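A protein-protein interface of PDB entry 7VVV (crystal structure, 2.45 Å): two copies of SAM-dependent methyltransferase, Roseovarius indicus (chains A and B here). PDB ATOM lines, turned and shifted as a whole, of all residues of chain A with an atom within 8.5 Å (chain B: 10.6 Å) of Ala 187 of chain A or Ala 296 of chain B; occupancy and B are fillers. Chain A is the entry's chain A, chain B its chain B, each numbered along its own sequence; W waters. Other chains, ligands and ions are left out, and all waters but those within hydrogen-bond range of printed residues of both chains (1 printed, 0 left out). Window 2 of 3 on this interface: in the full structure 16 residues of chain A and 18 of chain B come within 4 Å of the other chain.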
ATOM      1  N   ILE A 103     -18.561  -9.811  23.300  1.00  0.00           N
ATOM      2  CA  ILE A 103     -17.650 -10.900  23.042  1.00  0.00           C
ATOM      3  C   ILE A 103     -16.331 -10.665  23.733  1.00  0.00           C
ATOM      4  O   ILE A 103     -15.329 -11.107  23.305  1.00  0.00           O
ATOM      5  CB  ILE A 103     -17.392 -11.145  21.557  1.00  0.00           C
ATOM      6  CG1 ILE A 103     -16.799  -9.957  20.885  1.00  0.00           C
ATOM      7  CG2 ILE A 103     -18.652 -11.419  20.823  1.00  0.00           C
ATOM      8  CD1 ILE A 103     -16.412 -10.276  19.475  1.00  0.00           C
ATOM      9  N   ARG A 109     -13.533 -14.192  21.835  1.00  0.00           N
ATOM     10  CA  ARG A 109     -12.988 -13.610  20.635  1.00  0.00           C
ATOM     11  C   ARG A 109     -12.421 -14.660  19.738  1.00  0.00           C
ATOM     12  O   ARG A 109     -12.540 -14.614  18.553  1.00  0.00           O
ATOM     13  CB  ARG A 109     -11.920 -12.623  20.983  1.00  0.00           C
ATOM     14  CG  ARG A 109     -12.440 -11.310  21.468  1.00  0.00           C
ATOM     15  CD  ARG A 109     -11.344 -10.433  21.937  1.00  0.00           C
ATOM     16  NE  ARG A 109     -11.829  -9.387  22.776  1.00  0.00           N
ATOM     17  CZ  ARG A 109     -11.568  -9.306  24.053  1.00  0.00           C
ATOM     18  NH1 ARG A 109     -10.850 -10.199  24.612  1.00  0.00           N
ATOM     19  NH2 ARG A 109     -12.015  -8.336  24.770  1.00  0.00           N
ATOM     20  N   VAL A 112     -15.265 -16.200  17.953  1.00  0.00           N
ATOM     21  CA  VAL A 112     -15.819 -15.260  16.980  1.00  0.00           C
ATOM     22  C   VAL A 112     -14.913 -15.168  15.756  1.00  0.00           C
ATOM     23  O   VAL A 112     -15.388 -15.175  14.609  1.00  0.00           O
ATOM     24  CB  VAL A 112     -16.037 -13.879  17.633  1.00  0.00           C
ATOM     25  CG1 VAL A 112     -16.325 -12.824  16.580  1.00  0.00           C
ATOM     26  CG2 VAL A 112     -17.165 -13.929  18.651  1.00  0.00           C
ATOM     27  N   GLY A 113     -13.593 -15.100  15.979  1.00  0.00           N
ATOM     28  CA  GLY A 113     -12.660 -15.032  14.861  1.00  0.00           C
ATOM     29  C   GLY A 113     -12.732 -16.229  13.929  1.00  0.00           C
ATOM     30  O   GLY A 113     -12.378 -16.125  12.751  1.00  0.00           O
ATOM     31  N   LEU A 181     -21.125  -3.742  19.120  1.00  0.00           N
ATOM     32  CA  LEU A 181     -20.844  -5.090  18.758  1.00  0.00           C
ATOM     33  C   LEU A 181     -20.267  -5.074  17.399  1.00  0.00           C
ATOM     34  O   LEU A 181     -19.465  -5.876  17.130  1.00  0.00           O
ATOM     35  CB  LEU A 181     -22.057  -5.950  18.829  1.00  0.00           C
ATOM     36  CG  LEU A 181     -21.958  -7.260  18.109  1.00  0.00           C
ATOM     37  CD1 LEU A 181     -21.113  -8.227  18.846  1.00  0.00           C
ATOM     38  CD2 LEU A 181     -23.276  -7.901  17.839  1.00  0.00           C
ATOM     39  N   LEU A 182     -20.682  -4.146  16.554  1.00  0.00           N
ATOM     40  CA  LEU A 182     -20.149  -4.035  15.192  1.00  0.00           C
ATOM     41  C   LEU A 182     -18.694  -3.576  15.204  1.00  0.00           C
ATOM     42  O   LEU A 182     -17.885  -4.036  14.389  1.00  0.00           O
ATOM     43  CB  LEU A 182     -21.003  -3.078  14.360  1.00  0.00           C
ATOM     44  CG  LEU A 182     -22.435  -3.514  13.990  1.00  0.00           C
ATOM     45  CD1 LEU A 182     -23.019  -2.578  12.966  1.00  0.00           C
ATOM     46  CD2 LEU A 182     -22.461  -4.945  13.456  1.00  0.00           C
ATOM     47  N   ARG A 183     -18.330  -2.676  16.127  1.00  0.00           N
ATOM     48  CA  ARG A 183     -16.914  -2.349  16.261  1.00  0.00           C
ATOM     49  C   ARG A 183     -16.115  -3.592  16.623  1.00  0.00           C
ATOM     50  O   ARG A 183     -14.995  -3.775  16.147  1.00  0.00           O
ATOM     51  CB  ARG A 183     -16.703  -1.270  17.316  1.00  0.00           C
ATOM     52  CG  ARG A 183     -17.591  -0.063  17.149  1.00  0.00           C
ATOM     53  CD  ARG A 183     -17.098   0.787  16.010  1.00  0.00           C
ATOM     54  NE  ARG A 183     -17.939   1.966  15.857  1.00  0.00           N
ATOM     55  CZ  ARG A 183     -17.718   3.134  16.460  1.00  0.00           C
ATOM     56  NH1 ARG A 183     -16.663   3.306  17.247  1.00  0.00           N
ATOM     57  NH2 ARG A 183     -18.557   4.142  16.267  1.00  0.00           N
ATOM     58  N   ARG A 184     -16.698  -4.482  17.376  1.00  0.00           N
ATOM     59  CA  ARG A 184     -15.996  -5.656  17.731  1.00  0.00           C
ATOM     60  C   ARG A 184     -15.885  -6.657  16.640  1.00  0.00           C
ATOM     61  O   ARG A 184     -14.847  -7.144  16.404  1.00  0.00           O
ATOM     62  CB  ARG A 184     -16.591  -6.287  18.953  1.00  0.00           C
ATOM     63  CG  ARG A 184     -16.235  -5.610  20.227  1.00  0.00           C
ATOM     64  CD  ARG A 184     -17.437  -5.575  21.098  1.00  0.00           C
ATOM     65  NE  ARG A 184     -17.192  -5.272  22.470  1.00  0.00           N
ATOM     66  CZ  ARG A 184     -17.152  -4.077  22.980  1.00  0.00           C
ATOM     67  NH1 ARG A 184     -17.263  -3.040  22.244  1.00  0.00           N
ATOM     68  NH2 ARG A 184     -16.947  -3.938  24.233  1.00  0.00           N
ATOM     69  N   THR A 185     -16.965  -6.968  15.970  1.00  0.00           N
ATOM     70  CA  THR A 185     -16.933  -7.950  14.913  1.00  0.00           C
ATOM     71  C   THR A 185     -16.017  -7.609  13.782  1.00  0.00           C
ATOM     72  O   THR A 185     -15.376  -8.445  13.249  1.00  0.00           O
ATOM     73  CB  THR A 185     -18.304  -8.230  14.350  1.00  0.00           C
ATOM     74  OG1 THR A 185     -18.877  -7.036  13.868  1.00  0.00           O
ATOM     75  CG2 THR A 185     -19.126  -8.767  15.354  1.00  0.00           C
ATOM     76  N   ARG A 186     -15.979  -6.356  13.423  1.00  0.00           N
ATOM     77  CA  ARG A 186     -15.162  -5.932  12.339  1.00  0.00           C
ATOM     78  C   ARG A 186     -13.704  -6.139  12.580  1.00  0.00           C
ATOM     79  O   ARG A 186     -12.971  -6.405  11.696  1.00  0.00           O
ATOM     80  CB  ARG A 186     -15.411  -4.493  12.029  1.00  0.00           C
ATOM     81  CG  ARG A 186     -14.748  -4.083  10.765  1.00  0.00           C
ATOM     82  CD  ARG A 186     -15.397  -2.923  10.101  1.00  0.00           C
ATOM     83  NE  ARG A 186     -14.364  -2.111   9.555  1.00  0.00           N
ATOM     84  CZ  ARG A 186     -13.949  -1.012  10.121  1.00  0.00           C
ATOM     85  NH1 ARG A 186     -12.956  -0.327   9.602  1.00  0.00           N
ATOM     86  NH2 ARG A 186     -14.532  -0.592  11.212  1.00  0.00           N
ATOM     87  N   ALA A 187     -13.305  -6.007  13.810  1.00  0.00           N
ATOM     88  CA  ALA A 187     -11.895  -6.135  14.150  1.00  0.00           C
ATOM     89  C   ALA A 187     -11.508  -7.589  14.408  1.00  0.00           C
ATOM     90  O   ALA A 187     -10.459  -8.035  13.943  1.00  0.00           O
ATOM     91  CB  ALA A 187     -11.567  -5.262  15.367  1.00  0.00           C
ATOM     92  N   THR A 188     -12.322  -8.364  15.132  1.00  0.00           N
ATOM     93  CA  THR A 188     -11.857  -9.719  15.391  1.00  0.00           C
ATOM     94  C   THR A 188     -12.354 -10.726  14.346  1.00  0.00           C
ATOM     95  O   THR A 188     -11.785 -11.818  14.254  1.00  0.00           O
ATOM     96  CB  THR A 188     -12.220 -10.181  16.835  1.00  0.00           C
ATOM     97  OG1 THR A 188     -13.520 -10.753  16.884  1.00  0.00           O
ATOM     98  CG2 THR A 188     -12.171  -9.022  17.832  1.00  0.00           C
ATOM     99  N   ALA A 189     -13.370 -10.400  13.540  1.00  0.00           N
ATOM    100  CA  ALA A 189     -13.783 -11.263  12.423  1.00  0.00           C
ATOM    101  C   ALA A 189     -14.143 -10.437  11.190  1.00  0.00           C
ATOM    102  O   ALA A 189     -15.311 -10.345  10.801  1.00  0.00           O
ATOM    103  CB  ALA A 189     -14.954 -12.159  12.826  1.00  0.00           C
ATOM    104  N   PRO A 190     -13.140  -9.866  10.515  1.00  0.00           N
ATOM    105  CA  PRO A 190     -13.427  -8.912   9.420  1.00  0.00           C
ATOM    106  C   PRO A 190     -14.132  -9.498   8.214  1.00  0.00           C
ATOM    107  O   PRO A 190     -14.682  -8.725   7.414  1.00  0.00           O
ATOM    108  CB  PRO A 190     -12.034  -8.391   9.029  1.00  0.00           C
ATOM    109  CG  PRO A 190     -11.070  -9.340   9.649  1.00  0.00           C
ATOM    110  CD  PRO A 190     -11.718  -9.851  10.893  1.00  0.00           C
ATOM    111  N   ALA A 191     -14.137 -10.814   8.024  1.00  0.00           N
ATOM    112  CA  ALA A 191     -14.861 -11.383   6.889  1.00  0.00           C
ATOM    113  C   ALA A 191     -16.210 -11.980   7.276  1.00  0.00           C
ATOM    114  O   ALA A 191     -16.929 -12.471   6.397  1.00  0.00           O
ATOM    115  CB  ALA A 191     -14.007 -12.444   6.186  1.00  0.00           C
ATOM    116  N   ASN A 214     -20.185   1.461   9.841  1.00  0.00           N
ATOM    117  CA  ASN A 214     -19.249   0.605  10.557  1.00  0.00           C
ATOM    118  C   ASN A 214     -18.691  -0.485   9.646  1.00  0.00           C
ATOM    119  O   ASN A 214     -18.311  -1.553  10.122  1.00  0.00           O
ATOM    120  CB  ASN A 214     -19.918  -0.017  11.787  1.00  0.00           C
ATOM    121  CG  ASN A 214     -20.171   0.991  12.905  1.00  0.00           C
ATOM    122  OD1 ASN A 214     -19.287   1.273  13.722  1.00  0.00           O
ATOM    123  ND2 ASN A 214     -21.398   1.500  12.980  1.00  0.00           N
ATOM    124  N   TYR A 216     -20.098  -2.249   6.923  1.00  0.00           N
ATOM    125  CA  TYR A 216     -20.931  -3.369   6.509  1.00  0.00           C
ATOM    126  C   TYR A 216     -21.959  -2.889   5.495  1.00  0.00           C
ATOM    127  O   TYR A 216     -22.489  -1.779   5.623  1.00  0.00           O
ATOM    128  CB  TYR A 216     -21.659  -4.010   7.720  1.00  0.00           C
ATOM    129  CG  TYR A 216     -20.762  -4.745   8.691  1.00  0.00           C
ATOM    130  CD1 TYR A 216     -20.423  -6.075   8.487  1.00  0.00           C
ATOM    131  CD2 TYR A 216     -20.267  -4.112   9.824  1.00  0.00           C
ATOM    132  CE1 TYR A 216     -19.596  -6.757   9.385  1.00  0.00           C
ATOM    133  CE2 TYR A 216     -19.447  -4.777  10.712  1.00  0.00           C
ATOM    134  CZ  TYR A 216     -19.122  -6.098  10.491  1.00  0.00           C
ATOM    135  OH  TYR A 216     -18.307  -6.747  11.383  1.00  0.00           O
ATOM    136  N   ARG B 186      -4.351   2.909  14.421  1.00  0.00           N
ATOM    137  CA  ARG B 186      -4.967   1.793  13.759  1.00  0.00           C
ATOM    138  C   ARG B 186      -4.806   1.808  12.266  1.00  0.00           C
ATOM    139  O   ARG B 186      -4.849   0.802  11.614  1.00  0.00           O
ATOM    140  CB  ARG B 186      -6.426   1.740  14.102  1.00  0.00           C
ATOM    141  CG  ARG B 186      -7.110   0.497  13.646  1.00  0.00           C
ATOM    142  CD  ARG B 186      -8.580   0.710  13.572  1.00  0.00           C
ATOM    143  NE  ARG B 186      -9.270  -0.543  13.441  1.00  0.00           N
ATOM    144  CZ  ARG B 186     -10.571  -0.698  13.558  1.00  0.00           C
ATOM    145  NH1 ARG B 186     -11.304   0.339  13.843  1.00  0.00           N
ATOM    146  NH2 ARG B 186     -11.137  -1.879  13.406  1.00  0.00           N
ATOM    147  N   ALA B 189      -0.270   1.950  11.785  1.00  0.00           N
ATOM    148  CA  ALA B 189       0.476   0.826  12.308  1.00  0.00           C
ATOM    149  C   ALA B 189      -0.487  -0.187  12.854  1.00  0.00           C
ATOM    150  O   ALA B 189      -0.583  -0.364  14.027  1.00  0.00           O
ATOM    151  CB  ALA B 189       1.409   1.319  13.382  1.00  0.00           C
ATOM    152  N   PRO B 190      -1.236  -0.859  11.915  1.00  0.00           N
ATOM    153  CA  PRO B 190      -2.246  -1.762  12.453  1.00  0.00           C
ATOM    154  C   PRO B 190      -1.907  -2.949  13.266  1.00  0.00           C
ATOM    155  O   PRO B 190      -2.769  -3.561  13.756  1.00  0.00           O
ATOM    156  CB  PRO B 190      -3.004  -2.197  11.237  1.00  0.00           C
ATOM    157  CG  PRO B 190      -2.065  -2.154  10.190  1.00  0.00           C
ATOM    158  CD  PRO B 190      -1.380  -0.902  10.404  1.00  0.00           C
ATOM    159  N   ALA B 191      -0.671  -3.271  13.398  1.00  0.00           N
ATOM    160  CA  ALA B 191      -0.217  -4.432  14.145  1.00  0.00           C
ATOM    161  C   ALA B 191       0.435  -4.055  15.470  1.00  0.00           C
ATOM    162  O   ALA B 191       0.754  -4.946  16.264  1.00  0.00           O
ATOM    163  CB  ALA B 191       0.754  -5.247  13.278  1.00  0.00           C
ATOM    164  N   ALA B 192       0.617  -2.763  15.733  1.00  0.00           N
ATOM    165  CA  ALA B 192       1.309  -2.306  16.925  1.00  0.00           C
ATOM    166  C   ALA B 192       0.382  -2.234  18.139  1.00  0.00           C
ATOM    167  O   ALA B 192      -0.806  -1.920  18.028  1.00  0.00           O
ATOM    168  CB  ALA B 192       1.921  -0.926  16.666  1.00  0.00           C
ATOM    169  N   ASP B 193       0.944  -2.514  19.310  1.00  0.00           N
ATOM    170  CA  ASP B 193       0.274  -2.188  20.556  1.00  0.00           C
ATOM    171  C   ASP B 193       0.282  -0.684  20.770  1.00  0.00           C
ATOM    172  O   ASP B 193       1.187   0.023  20.309  1.00  0.00           O
ATOM    173  CB  ASP B 193       0.970  -2.844  21.750  1.00  0.00           C
ATOM    174  CG  ASP B 193       1.032  -4.340  21.647  1.00  0.00           C
ATOM    175  OD1 ASP B 193       0.160  -4.924  20.975  1.00  0.00           O
ATOM    176  OD2 ASP B 193       1.974  -4.935  22.230  1.00  0.00           O
ATOM    177  N   VAL B 194      -0.717  -0.206  21.520  1.00  0.00           N
ATOM    178  CA  VAL B 194      -0.790   1.178  21.985  1.00  0.00           C
ATOM    179  C   VAL B 194      -0.953   1.151  23.505  1.00  0.00           C
ATOM    180  O   VAL B 194      -1.838   0.468  24.028  1.00  0.00           O
ATOM    181  CB  VAL B 194      -1.943   1.952  21.305  1.00  0.00           C
ATOM    182  CG1 VAL B 194      -1.990   3.412  21.773  1.00  0.00           C
ATOM    183  CG2 VAL B 194      -1.777   1.911  19.780  1.00  0.00           C
ATOM    184  N   PHE B 211     -10.989   1.631  23.902  1.00  0.00           N
ATOM    185  CA  PHE B 211     -10.207   0.751  23.031  1.00  0.00           C
ATOM    186  C   PHE B 211     -11.110  -0.165  22.214  1.00  0.00           C
ATOM    187  O   PHE B 211     -10.930  -0.309  21.003  1.00  0.00           O
ATOM    188  CB  PHE B 211      -9.218  -0.096  23.851  1.00  0.00           C
ATOM    189  CG  PHE B 211      -8.084   0.692  24.428  1.00  0.00           C
ATOM    190  CD1 PHE B 211      -8.217   1.319  25.655  1.00  0.00           C
ATOM    191  CD2 PHE B 211      -6.882   0.811  23.743  1.00  0.00           C
ATOM    192  CE1 PHE B 211      -7.166   2.049  26.192  1.00  0.00           C
ATOM    193  CE2 PHE B 211      -5.847   1.547  24.259  1.00  0.00           C
ATOM    194  CZ  PHE B 211      -5.979   2.164  25.490  1.00  0.00           C
ATOM    195  N   GLU B 212     -12.068  -0.814  22.868  1.00  0.00           N
ATOM    196  CA  GLU B 212     -12.934  -1.755  22.170  1.00  0.00           C
ATOM    197  C   GLU B 212     -13.685  -1.074  21.028  1.00  0.00           C
ATOM    198  O   GLU B 212     -13.877  -1.669  19.967  1.00  0.00           O
ATOM    199  CB  GLU B 212     -13.913  -2.383  23.164  1.00  0.00           C
ATOM    200  CG  GLU B 212     -13.264  -3.372  24.142  1.00  0.00           C
ATOM    201  CD  GLU B 212     -13.093  -4.746  23.511  1.00  0.00           C
ATOM    202  OE1 GLU B 212     -13.378  -4.886  22.309  1.00  0.00           O
ATOM    203  OE2 GLU B 212     -12.712  -5.701  24.215  1.00  0.00           O
ATOM    204  N   ALA B 213     -14.110   0.175  21.224  1.00  0.00           N
ATOM    205  CA  ALA B 213     -14.801   0.892  20.164  1.00  0.00           C
ATOM    206  C   ALA B 213     -13.898   1.139  18.960  1.00  0.00           C
ATOM    207  O   ALA B 213     -14.405   1.436  17.870  1.00  0.00           O
ATOM    208  CB  ALA B 213     -15.328   2.232  20.683  1.00  0.00           C
ATOM    209  N   ASN B 214     -12.573   1.010  19.122  1.00  0.00           N
ATOM    210  CA  ASN B 214     -11.656   1.471  18.086  1.00  0.00           C
ATOM    211  C   ASN B 214     -10.676   0.397  17.634  1.00  0.00           C
ATOM    212  O   ASN B 214      -9.590   0.732  17.172  1.00  0.00           O
ATOM    213  CB  ASN B 214     -10.900   2.714  18.560  1.00  0.00           C
ATOM    214  CG  ASN B 214     -11.793   3.934  18.607  1.00  0.00           C
ATOM    215  OD1 ASN B 214     -12.206   4.451  17.551  1.00  0.00           O
ATOM    216  ND2 ASN B 214     -12.159   4.371  19.823  1.00  0.00           N
ATOM    217  N   GLY B 215     -11.028  -0.880  17.754  1.00  0.00           N
ATOM    218  CA  GLY B 215     -10.249  -1.932  17.139  1.00  0.00           C
ATOM    219  C   GLY B 215      -9.200  -2.598  18.005  1.00  0.00           C
ATOM    220  O   GLY B 215      -8.416  -3.395  17.472  1.00  0.00           O
ATOM    221  N   TYR B 216      -9.191  -2.345  19.326  1.00  0.00           N
ATOM    222  CA  TYR B 216      -8.139  -2.818  20.225  1.00  0.00           C
ATOM    223  C   TYR B 216      -8.732  -3.543  21.429  1.00  0.00           C
ATOM    224  O   TYR B 216      -9.698  -3.070  22.036  1.00  0.00           O
ATOM    225  CB  TYR B 216      -7.280  -1.663  20.752  1.00  0.00           C
ATOM    226  CG  TYR B 216      -6.487  -0.904  19.720  1.00  0.00           C
ATOM    227  CD1 TYR B 216      -5.199  -1.314  19.379  1.00  0.00           C
ATOM    228  CD2 TYR B 216      -6.998   0.240  19.109  1.00  0.00           C
ATOM    229  CE1 TYR B 216      -4.445  -0.626  18.461  1.00  0.00           C
ATOM    230  CE2 TYR B 216      -6.242   0.940  18.179  1.00  0.00           C
ATOM    231  CZ  TYR B 216      -4.959   0.497  17.862  1.00  0.00           C
ATOM    232  OH  TYR B 216      -4.169   1.163  16.941  1.00  0.00           O
ATOM    233  N   VAL B 217      -8.140  -4.680  21.778  1.00  0.00           N
ATOM    234  CA  VAL B 217      -8.459  -5.384  23.016  1.00  0.00           C
ATOM    235  C   VAL B 217      -7.667  -4.735  24.142  1.00  0.00           C
ATOM    236  O   VAL B 217      -6.432  -4.738  24.094  1.00  0.00           O
ATOM    237  CB  VAL B 217      -8.130  -6.878  22.896  1.00  0.00           C
ATOM    238  CG1 VAL B 217      -8.519  -7.625  24.156  1.00  0.00           C
ATOM    239  CG2 VAL B 217      -8.830  -7.449  21.674  1.00  0.00           C
ATOM    240  N   PRO B 218      -8.299  -4.234  25.171  1.00  0.00           N
ATOM    241  CA  PRO B 218      -7.563  -3.607  26.258  1.00  0.00           C
ATOM    242  C   PRO B 218      -7.147  -4.500  27.397  1.00  0.00           C
ATOM    243  O   PRO B 218      -7.754  -5.460  27.693  1.00  0.00           O
ATOM    244  CB  PRO B 218      -8.539  -2.601  26.782  1.00  0.00           C
ATOM    245  CG  PRO B 218      -9.827  -3.134  26.455  1.00  0.00           C
ATOM    246  CD  PRO B 218      -9.715  -3.906  25.218  1.00  0.00           C
ATOM    247  N   ARG B 292      -3.005  -1.084  27.877  1.00  0.00           N
ATOM    248  CA  ARG B 292      -2.481  -1.458  26.580  1.00  0.00           C
ATOM    249  C   ARG B 292      -3.631  -1.929  25.708  1.00  0.00           C
ATOM    250  O   ARG B 292      -4.455  -2.749  26.143  1.00  0.00           O
ATOM    251  CB  ARG B 292      -1.432  -2.555  26.711  1.00  0.00           C
ATOM    252  CG  ARG B 292      -1.071  -3.201  25.397  1.00  0.00           C
ATOM    253  CD  ARG B 292      -0.777  -4.661  25.613  1.00  0.00           C
ATOM    254  NE  ARG B 292       0.638  -4.848  25.831  1.00  0.00           N
ATOM    255  CZ  ARG B 292       1.170  -5.712  26.694  1.00  0.00           C
ATOM    256  NH1 ARG B 292       0.401  -6.497  27.436  1.00  0.00           N
ATOM    257  NH2 ARG B 292       2.492  -5.779  26.809  1.00  0.00           N
ATOM    258  N   GLY B 293      -3.706  -1.381  24.498  1.00  0.00           N
ATOM    259  CA  GLY B 293      -4.592  -1.883  23.475  1.00  0.00           C
ATOM    260  C   GLY B 293      -3.796  -2.699  22.464  1.00  0.00           C
ATOM    261  O   GLY B 293      -2.813  -2.220  21.894  1.00  0.00           O
ATOM    262  N   ARG B 294      -4.252  -3.920  22.250  1.00  0.00           N
ATOM    263  CA  ARG B 294      -3.605  -4.856  21.353  1.00  0.00           C
ATOM    264  C   ARG B 294      -4.558  -5.168  20.206  1.00  0.00           C
ATOM    265  O   ARG B 294      -5.685  -5.629  20.457  1.00  0.00           O
ATOM    266  CB  ARG B 294      -3.236  -6.125  22.127  1.00  0.00           C
ATOM    267  CG  ARG B 294      -2.562  -7.220  21.318  1.00  0.00           C
ATOM    268  CD  ARG B 294      -1.738  -8.123  22.248  1.00  0.00           C
ATOM    269  NE  ARG B 294      -0.401  -7.567  22.452  1.00  0.00           N
ATOM    270  CZ  ARG B 294       0.378  -7.818  23.504  1.00  0.00           C
ATOM    271  NH1 ARG B 294      -0.040  -8.616  24.481  1.00  0.00           N
ATOM    272  NH2 ARG B 294       1.577  -7.251  23.588  1.00  0.00           N
ATOM    273  N   PRO B 295      -4.170  -4.951  18.950  1.00  0.00           N
ATOM    274  CA  PRO B 295      -5.068  -5.268  17.835  1.00  0.00           C
ATOM    275  C   PRO B 295      -5.260  -6.772  17.712  1.00  0.00           C
ATOM    276  O   PRO B 295      -4.462  -7.567  18.208  1.00  0.00           O
ATOM    277  CB  PRO B 295      -4.329  -4.712  16.613  1.00  0.00           C
ATOM    278  CG  PRO B 295      -3.066  -4.035  17.161  1.00  0.00           C
ATOM    279  CD  PRO B 295      -2.811  -4.640  18.487  1.00  0.00           C
ATOM    280  N   ALA B 296      -6.313  -7.160  16.998  1.00  0.00           N
ATOM    281  CA  ALA B 296      -6.699  -8.574  16.829  1.00  0.00           C
ATOM    282  C   ALA B 296      -5.688  -9.481  16.097  1.00  0.00           C
ATOM    283  O   ALA B 296      -4.629  -9.052  15.629  1.00  0.00           O
ATOM    284  CB  ALA B 296      -8.023  -8.637  16.107  1.00  0.00           C
HETATM  285  O   HOH W   1     -13.915  -7.378  22.310  1.00  0.00           O
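Of the printed residues of chain B, Ala 187 of chain A touches Arg 186, Gly 215 and Ala 296.
No residue of chain B comes within 4 Å of Thr 188 of chain A.
No residue of chain B comes within 4 Å of Ala 189 of chain A.
Of the printed residues of chain A, Ala 213 of chain B touches Arg 183 (3.0 Å).
Of the printed residues of chain B, Arg 109 of chain A touches Glu 212 (2.8 Å) and Val 217 (3.5 Å).
Of the printed residues of chain A, Glu 212 of chain B touches Arg 109 (2.8 Å), Arg 183 (3.9 Å) and Arg 184 (3.5 Å).
Printed residues of chain A within 4 Å of Val 217 of chain B: Arg 109.
Printed residues of chain B within 4 Å of Arg 184 of chain A: Glu 212.
Tyr 216 of chain B touches none of the printed residues of chain A.
The nearest printed residue of chain B that does not touch Ala 187 of chain A is Tyr 216 of chain B (5.5 Å).
The nearest residue of chain A that does not touch Ala 296 of chain B is Thr 188 of chain A (4.05 Å).
The nearest printed residue of chain A that does not touch Gly 215 of chain B is Arg 183 of chain A (5.2 Å).
The guanidinium group (NH2) of Arg 109 of chain A lies within salt-bridge range of the side-chain carboxylate (OE2) of Glu 212 of chain B (2.8 Å).
NH1 of Arg 183 of chain A is in hydrogen-bond range of O of Ala 213 of chain B (3.0 Å).
The guanidinium group of Arg 184 of chain A is in salt-bridge range of the side-chain carboxylate of Glu 212 of chain B (3.8 Å).
Hydrophobic or aromatic side chains of chain B that line the printed part of chain A: Ala 213, Val 217 and Ala 296.
Among the printed residues, 8 pairs touch across the chains.
Among the printed residues, Asp or Glu carboxylates within 4 Å of a Lys or Arg side-chain nitrogen of the other chain: Arg 109 of chain A with Glu 212 of chain B (2.8 Å) and Arg 184 of chain A with Glu 212 of chain B (3.8 Å).
6 positions are printed for both chains.
Of the 8 pairs that touch across the chains among the printed residues, none has its exchanged pair printed and touching as well.
Water W1 lies within hydrogen-bond range of OE1 of Glu 212 of chain B (2.5 Å) and NE of Arg 109 of chain A (2.9 Å).
Among the printed residues, merely in contact across the chains: Ala 187 of chain A with Ala 296 of chain B (3.3 Å), Arg 109 of chain A with Val 217 of chain B (3.5 Å), Arg 183 of chain A with Glu 212 of chain B (3.9 Å), Ala 187 of chain A with Arg 186 of chain B (3.9 Å) and Ala 187 of chain A with Gly 215 of chain B (3.996 Å).
NE of Arg 183 of chain A is in hydrogen-bond range of OD1 of Asn 214 of chain A (2.6 Å).
The side-chain hydroxyl (OH) of Tyr 216 of chain B lies within hydrogen-bond range of the backbone NH (N) of Arg 186 of chain B.
N of Val 217 of chain B is in hydrogen-bond range of O of Arg 294 of chain B, at 2.9 Å.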
